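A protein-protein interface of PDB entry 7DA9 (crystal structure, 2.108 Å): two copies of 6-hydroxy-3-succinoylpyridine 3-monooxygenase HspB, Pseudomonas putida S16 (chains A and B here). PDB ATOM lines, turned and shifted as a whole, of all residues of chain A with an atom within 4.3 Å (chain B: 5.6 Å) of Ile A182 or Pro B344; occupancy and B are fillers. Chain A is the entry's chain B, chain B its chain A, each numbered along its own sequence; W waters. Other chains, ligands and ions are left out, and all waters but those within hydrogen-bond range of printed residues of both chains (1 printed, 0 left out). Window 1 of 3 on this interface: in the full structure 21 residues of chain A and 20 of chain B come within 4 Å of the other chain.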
ATOM      1  N   GLY A 181     -16.052  -2.064  15.502  1.00  0.00           N
ATOM      2  CA  GLY A 181     -14.779  -1.806  14.854  1.00  0.00           C
ATOM      3  C   GLY A 181     -14.155  -3.123  14.439  1.00  0.00           C
ATOM      4  O   GLY A 181     -14.860  -4.067  14.094  1.00  0.00           O
ATOM      5  N   ILE A 182     -12.819  -3.159  14.492  1.00  0.00           N
ATOM      6  CA  ILE A 182     -12.035  -4.299  14.044  1.00  0.00           C
ATOM      7  C   ILE A 182     -11.063  -4.691  15.145  1.00  0.00           C
ATOM      8  O   ILE A 182     -10.696  -3.884  15.998  1.00  0.00           O
ATOM      9  CB  ILE A 182     -11.261  -4.015  12.734  1.00  0.00           C
ATOM     10  CG1 ILE A 182     -10.284  -2.856  12.922  1.00  0.00           C
ATOM     11  CG2 ILE A 182     -12.223  -3.710  11.589  1.00  0.00           C
ATOM     12  CD1 ILE A 182      -9.068  -2.958  12.108  1.00  0.00           C
ATOM     13  N   THR A 183     -10.664  -5.958  15.122  1.00  0.00           N
ATOM     14  CA  THR A 183      -9.565  -6.476  15.930  1.00  0.00           C
ATOM     15  C   THR A 183      -8.444  -6.899  14.991  1.00  0.00           C
ATOM     16  O   THR A 183      -8.698  -7.599  14.008  1.00  0.00           O
ATOM     17  CB  THR A 183     -10.021  -7.665  16.768  1.00  0.00           C
ATOM     18  OG1 THR A 183     -11.081  -7.255  17.640  1.00  0.00           O
ATOM     19  CG2 THR A 183      -8.854  -8.258  17.573  1.00  0.00           C
ATOM     20  N   TRP A 184      -7.214  -6.481  15.284  1.00  0.00           N
ATOM     21  CA  TRP A 184      -6.111  -6.842  14.417  1.00  0.00           C
ATOM     22  C   TRP A 184      -5.799  -8.336  14.535  1.00  0.00           C
ATOM     23  O   TRP A 184      -6.009  -8.947  15.585  1.00  0.00           O
ATOM     24  CB  TRP A 184      -4.880  -6.002  14.755  1.00  0.00           C
ATOM     25  CG  TRP A 184      -5.055  -4.524  14.445  1.00  0.00           C
ATOM     26  CD1 TRP A 184      -5.494  -3.553  15.303  1.00  0.00           C
ATOM     27  CD2 TRP A 184      -4.811  -3.864  13.189  1.00  0.00           C
ATOM     28  NE1 TRP A 184      -5.520  -2.334  14.666  1.00  0.00           N
ATOM     29  CE2 TRP A 184      -5.099  -2.495  13.372  1.00  0.00           C
ATOM     30  CE3 TRP A 184      -4.356  -4.294  11.935  1.00  0.00           C
ATOM     31  CZ2 TRP A 184      -4.965  -1.553  12.345  1.00  0.00           C
ATOM     32  CZ3 TRP A 184      -4.224  -3.357  10.915  1.00  0.00           C
ATOM     33  CH2 TRP A 184      -4.526  -2.003  11.130  1.00  0.00           C
ATOM     34  N   HIS A 270      -7.248  -3.297  18.939  1.00  0.00           N
ATOM     35  CA  HIS A 270      -8.508  -2.976  18.274  1.00  0.00           C
ATOM     36  C   HIS A 270      -8.486  -1.557  17.718  1.00  0.00           C
ATOM     37  O   HIS A 270      -7.708  -0.705  18.155  1.00  0.00           O
ATOM     38  CB  HIS A 270      -9.700  -3.116  19.228  1.00  0.00           C
ATOM     39  CG  HIS A 270      -9.635  -4.323  20.121  1.00  0.00           C
ATOM     40  ND1 HIS A 270     -10.265  -5.510  19.814  1.00  0.00           N
ATOM     41  CD2 HIS A 270      -9.040  -4.515  21.324  1.00  0.00           C
ATOM     42  CE1 HIS A 270     -10.050  -6.387  20.784  1.00  0.00           C
ATOM     43  NE2 HIS A 270      -9.310  -5.805  21.714  1.00  0.00           N
ATOM     44  N   GLN A 271      -9.360  -1.317  16.735  1.00  0.00           N
ATOM     45  CA  GLN A 271      -9.766   0.027  16.326  1.00  0.00           C
ATOM     46  C   GLN A 271     -11.281   0.046  16.497  1.00  0.00           C
ATOM     47  O   GLN A 271     -12.013  -0.461  15.642  1.00  0.00           O
ATOM     48  CB  GLN A 271      -9.357   0.358  14.890  1.00  0.00           C
ATOM     49  CG  GLN A 271      -7.908   0.037  14.533  1.00  0.00           C
ATOM     50  CD  GLN A 271      -6.893   0.855  15.329  1.00  0.00           C
ATOM     51  OE1 GLN A 271      -5.908   0.317  15.838  1.00  0.00           O
ATOM     52  NE2 GLN A 271      -7.125   2.158  15.427  1.00  0.00           N
ATOM     53  N   ARG A 272     -11.758   0.587  17.615  1.00  0.00           N
ATOM     54  CA  ARG A 272     -13.184   0.559  17.920  1.00  0.00           C
ATOM     55  C   ARG A 272     -13.596   1.871  18.577  1.00  0.00           C
ATOM     56  O   ARG A 272     -12.783   2.546  19.215  1.00  0.00           O
ATOM     57  CB  ARG A 272     -13.541  -0.606  18.854  1.00  0.00           C
ATOM     58  CG  ARG A 272     -13.254  -1.976  18.295  1.00  0.00           C
ATOM     59  CD  ARG A 272     -13.621  -3.109  19.277  1.00  0.00           C
ATOM     60  NE  ARG A 272     -13.339  -4.383  18.620  1.00  0.00           N
ATOM     61  CZ  ARG A 272     -14.170  -4.992  17.778  1.00  0.00           C
ATOM     62  NH1 ARG A 272     -15.362  -4.458  17.512  1.00  0.00           N
ATOM     63  NH2 ARG A 272     -13.802  -6.129  17.185  1.00  0.00           N
ATOM     64  N   GLN B 271     -14.671   6.236   3.400  1.00  0.00           N
ATOM     65  CA  GLN B 271     -15.182   5.229   4.332  1.00  0.00           C
ATOM     66  C   GLN B 271     -15.857   6.018   5.446  1.00  0.00           C
ATOM     67  O   GLN B 271     -15.184   6.552   6.329  1.00  0.00           O
ATOM     68  CB  GLN B 271     -14.096   4.300   4.890  1.00  0.00           C
ATOM     69  CG  GLN B 271     -13.096   3.763   3.852  1.00  0.00           C
ATOM     70  CD  GLN B 271     -13.725   2.865   2.786  1.00  0.00           C
ATOM     71  OE1 GLN B 271     -13.386   2.986   1.607  1.00  0.00           O
ATOM     72  NE2 GLN B 271     -14.609   1.932   3.197  1.00  0.00           N
ATOM     73  N   PHE B 338     -21.672  -2.870   8.321  1.00  0.00           N
ATOM     74  CA  PHE B 338     -20.847  -1.931   7.562  1.00  0.00           C
ATOM     75  C   PHE B 338     -19.499  -1.700   8.247  1.00  0.00           C
ATOM     76  O   PHE B 338     -18.443  -1.802   7.619  1.00  0.00           O
ATOM     77  CB  PHE B 338     -21.557  -0.589   7.359  1.00  0.00           C
ATOM     78  CG  PHE B 338     -20.706   0.398   6.608  1.00  0.00           C
ATOM     79  CD1 PHE B 338     -20.585   0.312   5.232  1.00  0.00           C
ATOM     80  CD2 PHE B 338     -19.960   1.340   7.277  1.00  0.00           C
ATOM     81  CE1 PHE B 338     -19.753   1.186   4.529  1.00  0.00           C
ATOM     82  CE2 PHE B 338     -19.139   2.221   6.581  1.00  0.00           C
ATOM     83  CZ  PHE B 338     -19.038   2.133   5.198  1.00  0.00           C
ATOM     84  N   ILE B 339     -19.520  -1.373   9.537  1.00  0.00           N
ATOM     85  CA  ILE B 339     -18.301  -0.975  10.232  1.00  0.00           C
ATOM     86  C   ILE B 339     -17.374  -2.163  10.452  1.00  0.00           C
ATOM     87  O   ILE B 339     -16.144  -2.040  10.362  1.00  0.00           O
ATOM     88  CB  ILE B 339     -18.670  -0.313  11.567  1.00  0.00           C
ATOM     89  CG1 ILE B 339     -19.511   0.937  11.315  1.00  0.00           C
ATOM     90  CG2 ILE B 339     -17.416  -0.052  12.403  1.00  0.00           C
ATOM     91  CD1 ILE B 339     -20.133   1.492  12.595  1.00  0.00           C
ATOM     92  N   GLU B 340     -17.935  -3.317  10.786  1.00  0.00           N
ATOM     93  CA  GLU B 340     -17.100  -4.446  11.175  1.00  0.00           C
ATOM     94  C   GLU B 340     -16.725  -5.347  10.007  1.00  0.00           C
ATOM     95  O   GLU B 340     -15.687  -6.010  10.068  1.00  0.00           O
ATOM     96  CB  GLU B 340     -17.806  -5.260  12.263  1.00  0.00           C
ATOM     97  CG  GLU B 340     -18.192  -4.390  13.483  1.00  0.00           C
ATOM     98  CD  GLU B 340     -18.089  -5.151  14.818  1.00  0.00           C
ATOM     99  OE1 GLU B 340     -18.484  -6.340  14.854  1.00  0.00           O
ATOM    100  OE2 GLU B 340     -17.639  -4.561  15.836  1.00  0.00           O
ATOM    101  N   LEU B 341     -17.536  -5.405   8.949  1.00  0.00           N
ATOM    102  CA  LEU B 341     -17.264  -6.334   7.856  1.00  0.00           C
ATOM    103  C   LEU B 341     -17.004  -5.635   6.534  1.00  0.00           C
ATOM    104  O   LEU B 341     -15.962  -5.873   5.910  1.00  0.00           O
ATOM    105  CB  LEU B 341     -18.422  -7.326   7.695  1.00  0.00           C
ATOM    106  CG  LEU B 341     -18.640  -8.257   8.881  1.00  0.00           C
ATOM    107  CD1 LEU B 341     -19.834  -9.158   8.611  1.00  0.00           C
ATOM    108  CD2 LEU B 341     -17.371  -9.076   9.218  1.00  0.00           C
ATOM    109  N   VAL B 342     -17.906  -4.751   6.106  1.00  0.00           N
ATOM    110  CA  VAL B 342     -17.832  -4.206   4.752  1.00  0.00           C
ATOM    111  C   VAL B 342     -16.682  -3.221   4.626  1.00  0.00           C
ATOM    112  O   VAL B 342     -15.828  -3.344   3.739  1.00  0.00           O
ATOM    113  CB  VAL B 342     -19.165  -3.545   4.366  1.00  0.00           C
ATOM    114  CG1 VAL B 342     -19.031  -2.879   2.998  1.00  0.00           C
ATOM    115  CG2 VAL B 342     -20.270  -4.570   4.378  1.00  0.00           C
ATOM    116  N   SER B 343     -16.657  -2.210   5.490  1.00  0.00           N
ATOM    117  CA  SER B 343     -15.662  -1.160   5.328  1.00  0.00           C
ATOM    118  C   SER B 343     -14.230  -1.692   5.404  1.00  0.00           C
ATOM    119  O   SER B 343     -13.415  -1.298   4.551  1.00  0.00           O
ATOM    120  CB  SER B 343     -15.926  -0.049   6.349  1.00  0.00           C
ATOM    121  OG  SER B 343     -15.189   1.111   6.021  1.00  0.00           O
ATOM    122  N   PRO B 344     -13.862  -2.585   6.338  1.00  0.00           N
ATOM    123  CA  PRO B 344     -12.492  -3.144   6.301  1.00  0.00           C
ATOM    124  C   PRO B 344     -12.219  -3.964   5.055  1.00  0.00           C
ATOM    125  O   PRO B 344     -11.101  -3.919   4.515  1.00  0.00           O
ATOM    126  CB  PRO B 344     -12.416  -4.016   7.567  1.00  0.00           C
ATOM    127  CG  PRO B 344     -13.622  -3.628   8.406  1.00  0.00           C
ATOM    128  CD  PRO B 344     -14.660  -3.145   7.445  1.00  0.00           C
ATOM    129  N   ARG B 345     -13.216  -4.717   4.583  1.00  0.00           N
ATOM    130  CA  ARG B 345     -13.013  -5.562   3.409  1.00  0.00           C
ATOM    131  C   ARG B 345     -12.810  -4.715   2.166  1.00  0.00           C
ATOM    132  O   ARG B 345     -11.901  -4.971   1.365  1.00  0.00           O
ATOM    133  CB  ARG B 345     -14.198  -6.509   3.218  1.00  0.00           C
ATOM    134  CG  ARG B 345     -14.210  -7.219   1.866  1.00  0.00           C
ATOM    135  CD  ARG B 345     -12.930  -8.032   1.640  1.00  0.00           C
ATOM    136  NE  ARG B 345     -12.781  -9.170   2.543  1.00  0.00           N
ATOM    137  CZ  ARG B 345     -12.969 -10.447   2.199  1.00  0.00           C
ATOM    138  NH1 ARG B 345     -13.329 -10.781   0.964  1.00  0.00           N
ATOM    139  NH2 ARG B 345     -12.791 -11.399   3.104  1.00  0.00           N
ATOM    140  N   ALA B 346     -13.652  -3.697   1.984  1.00  0.00           N
ATOM    141  CA  ALA B 346     -13.505  -2.841   0.819  1.00  0.00           C
ATOM    142  C   ALA B 346     -12.183  -2.101   0.851  1.00  0.00           C
ATOM    143  O   ALA B 346     -11.577  -1.877  -0.199  1.00  0.00           O
ATOM    144  CB  ALA B 346     -14.665  -1.847   0.725  1.00  0.00           C
ATOM    145  N   SER B 347     -11.735  -1.693   2.052  1.00  0.00           N
ATOM    146  CA  SER B 347     -10.468  -0.967   2.192  1.00  0.00           C
ATOM    147  C   SER B 347      -9.289  -1.857   1.831  1.00  0.00           C
ATOM    148  O   SER B 347      -8.380  -1.434   1.110  1.00  0.00           O
ATOM    149  CB  SER B 347     -10.300  -0.427   3.627  1.00  0.00           C
ATOM    150  OG  SER B 347     -11.366   0.426   3.984  1.00  0.00           O
ATOM    151  N   ASP B 348      -9.286  -3.098   2.335  1.00  0.00           N
ATOM    152  CA  ASP B 348      -8.285  -4.070   1.894  1.00  0.00           C
ATOM    153  C   ASP B 348      -8.349  -4.314   0.380  1.00  0.00           C
ATOM    154  O   ASP B 348      -7.305  -4.450  -0.275  1.00  0.00           O
ATOM    155  CB  ASP B 348      -8.455  -5.377   2.668  1.00  0.00           C
ATOM    156  CG  ASP B 348      -7.949  -5.279   4.111  1.00  0.00           C
ATOM    157  OD1 ASP B 348      -8.286  -6.157   4.930  1.00  0.00           O
ATOM    158  OD2 ASP B 348      -7.214  -4.319   4.427  1.00  0.00           O
ATOM    159  N   ASN B 349      -9.565  -4.403  -0.186  1.00  0.00           N
ATOM    160  CA  ASN B 349      -9.713  -4.562  -1.635  1.00  0.00           C
ATOM    161  C   ASN B 349      -8.989  -3.449  -2.382  1.00  0.00           C
ATOM    162  O   ASN B 349      -8.202  -3.708  -3.301  1.00  0.00           O
ATOM    163  CB  ASN B 349     -11.189  -4.544  -2.050  1.00  0.00           C
ATOM    164  CG  ASN B 349     -11.941  -5.828  -1.701  1.00  0.00           C
ATOM    165  OD1 ASN B 349     -11.372  -6.797  -1.192  1.00  0.00           O
ATOM    166  ND2 ASN B 349     -13.248  -5.826  -1.978  1.00  0.00           N
ATOM    167  N   ARG B 351      -6.642  -1.385  -1.388  1.00  0.00           N
ATOM    168  CA  ARG B 351      -5.197  -1.403  -1.191  1.00  0.00           C
ATOM    169  C   ARG B 351      -4.543  -2.550  -1.951  1.00  0.00           C
ATOM    170  O   ARG B 351      -3.465  -2.377  -2.530  1.00  0.00           O
ATOM    171  CB  ARG B 351      -4.880  -1.482   0.309  1.00  0.00           C
ATOM    172  CG  ARG B 351      -5.180  -0.166   1.052  1.00  0.00           C
ATOM    173  CD  ARG B 351      -4.632  -0.151   2.481  1.00  0.00           C
ATOM    174  NE  ARG B 351      -5.439  -0.981   3.367  1.00  0.00           N
ATOM    175  CZ  ARG B 351      -6.192  -0.505   4.355  1.00  0.00           C
ATOM    176  NH1 ARG B 351      -6.235   0.805   4.588  1.00  0.00           N
ATOM    177  NH2 ARG B 351      -6.904  -1.341   5.103  1.00  0.00           N
HETATM  178  O   HOH W   1     -14.449  -6.543  12.918  1.00  0.00           O
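Printed residues of chain A that touch a printed residue of chain B: Gly A181, Ile A182 and Arg A272.
Hydrophobic or aromatic side chains of chain A that line the printed part of chain B: Ile A182.
Of the 14 printed residues of chain B, 3 touch a printed residue of chain A.
Printed residues of chain B that touch a printed residue of chain A: Ile B339, Glu B340 and Pro B344.
Among the printed residues, 4 pairs touch across the chains.
Water W1 lies within hydrogen-bond range of O of Gly A181 (2.8 Å) and O of Glu B340 (3.2 Å).
Of chain B, only Pro B344 (3.5 Å) comes within 4 Å of Ile A182.
Of chain A, only Ile A182 (3.5 Å) comes within 4 Å of Pro B344.
Of the printed residues of chain B, Gly A181 touches Ile B339 (3.9 Å) and Glu B340 (3.0 Å).
Of the printed residues of chain A, Ile B339 touches Gly A181 (3.9 Å).
The nearest printed residue of chain B that does not touch Ile A182 is Glu B340 (4.4 Å).
The nearest printed residue of chain A that does not touch Pro B344 is Gly A181 (5.8 Å).
The nearest printed residue of chain A that does not touch Glu B340 is Ile A182 (4.4 Å).
1 position is printed for both chains.
Of the 4 pairs that touch across the chains among the printed residues, none has its exchanged pair printed and touching as well.
NH1 of Arg A272 sits at hydrogen-bond distance from O of Gly A181 (3.5 Å).
The guanidinium group (NE) of Arg A272 lies within hydrogen-bond range of a ring nitrogen (ND1) of His A270, 3.5 Å away.
The backbone carbonyl oxygen (O) of Ile A182 sits at hydrogen-bond distance from the backbone NH (N) of Gln A271 (3.0 Å).
The side-chain hydroxyl (OG1) of Thr A183 sits at hydrogen-bond distance from the guanidinium group (NH2) of Arg A272 (3.0 Å).
The side-chain carboxylate (OE2) of Glu B340 is in salt-bridge range of the guanidinium group (NH1) of Arg A272, at 2.8 Å.
The backbone NH of Gly A181 sits at hydrogen-bond distance from the side-chain carboxylate of Glu B340 (3.0 Å).
Among the printed residues, merely in contact across the chains: Gly A181 with Ile B339 (3.9 Å) and Ile A182 with Pro B344 (3.5 Å).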
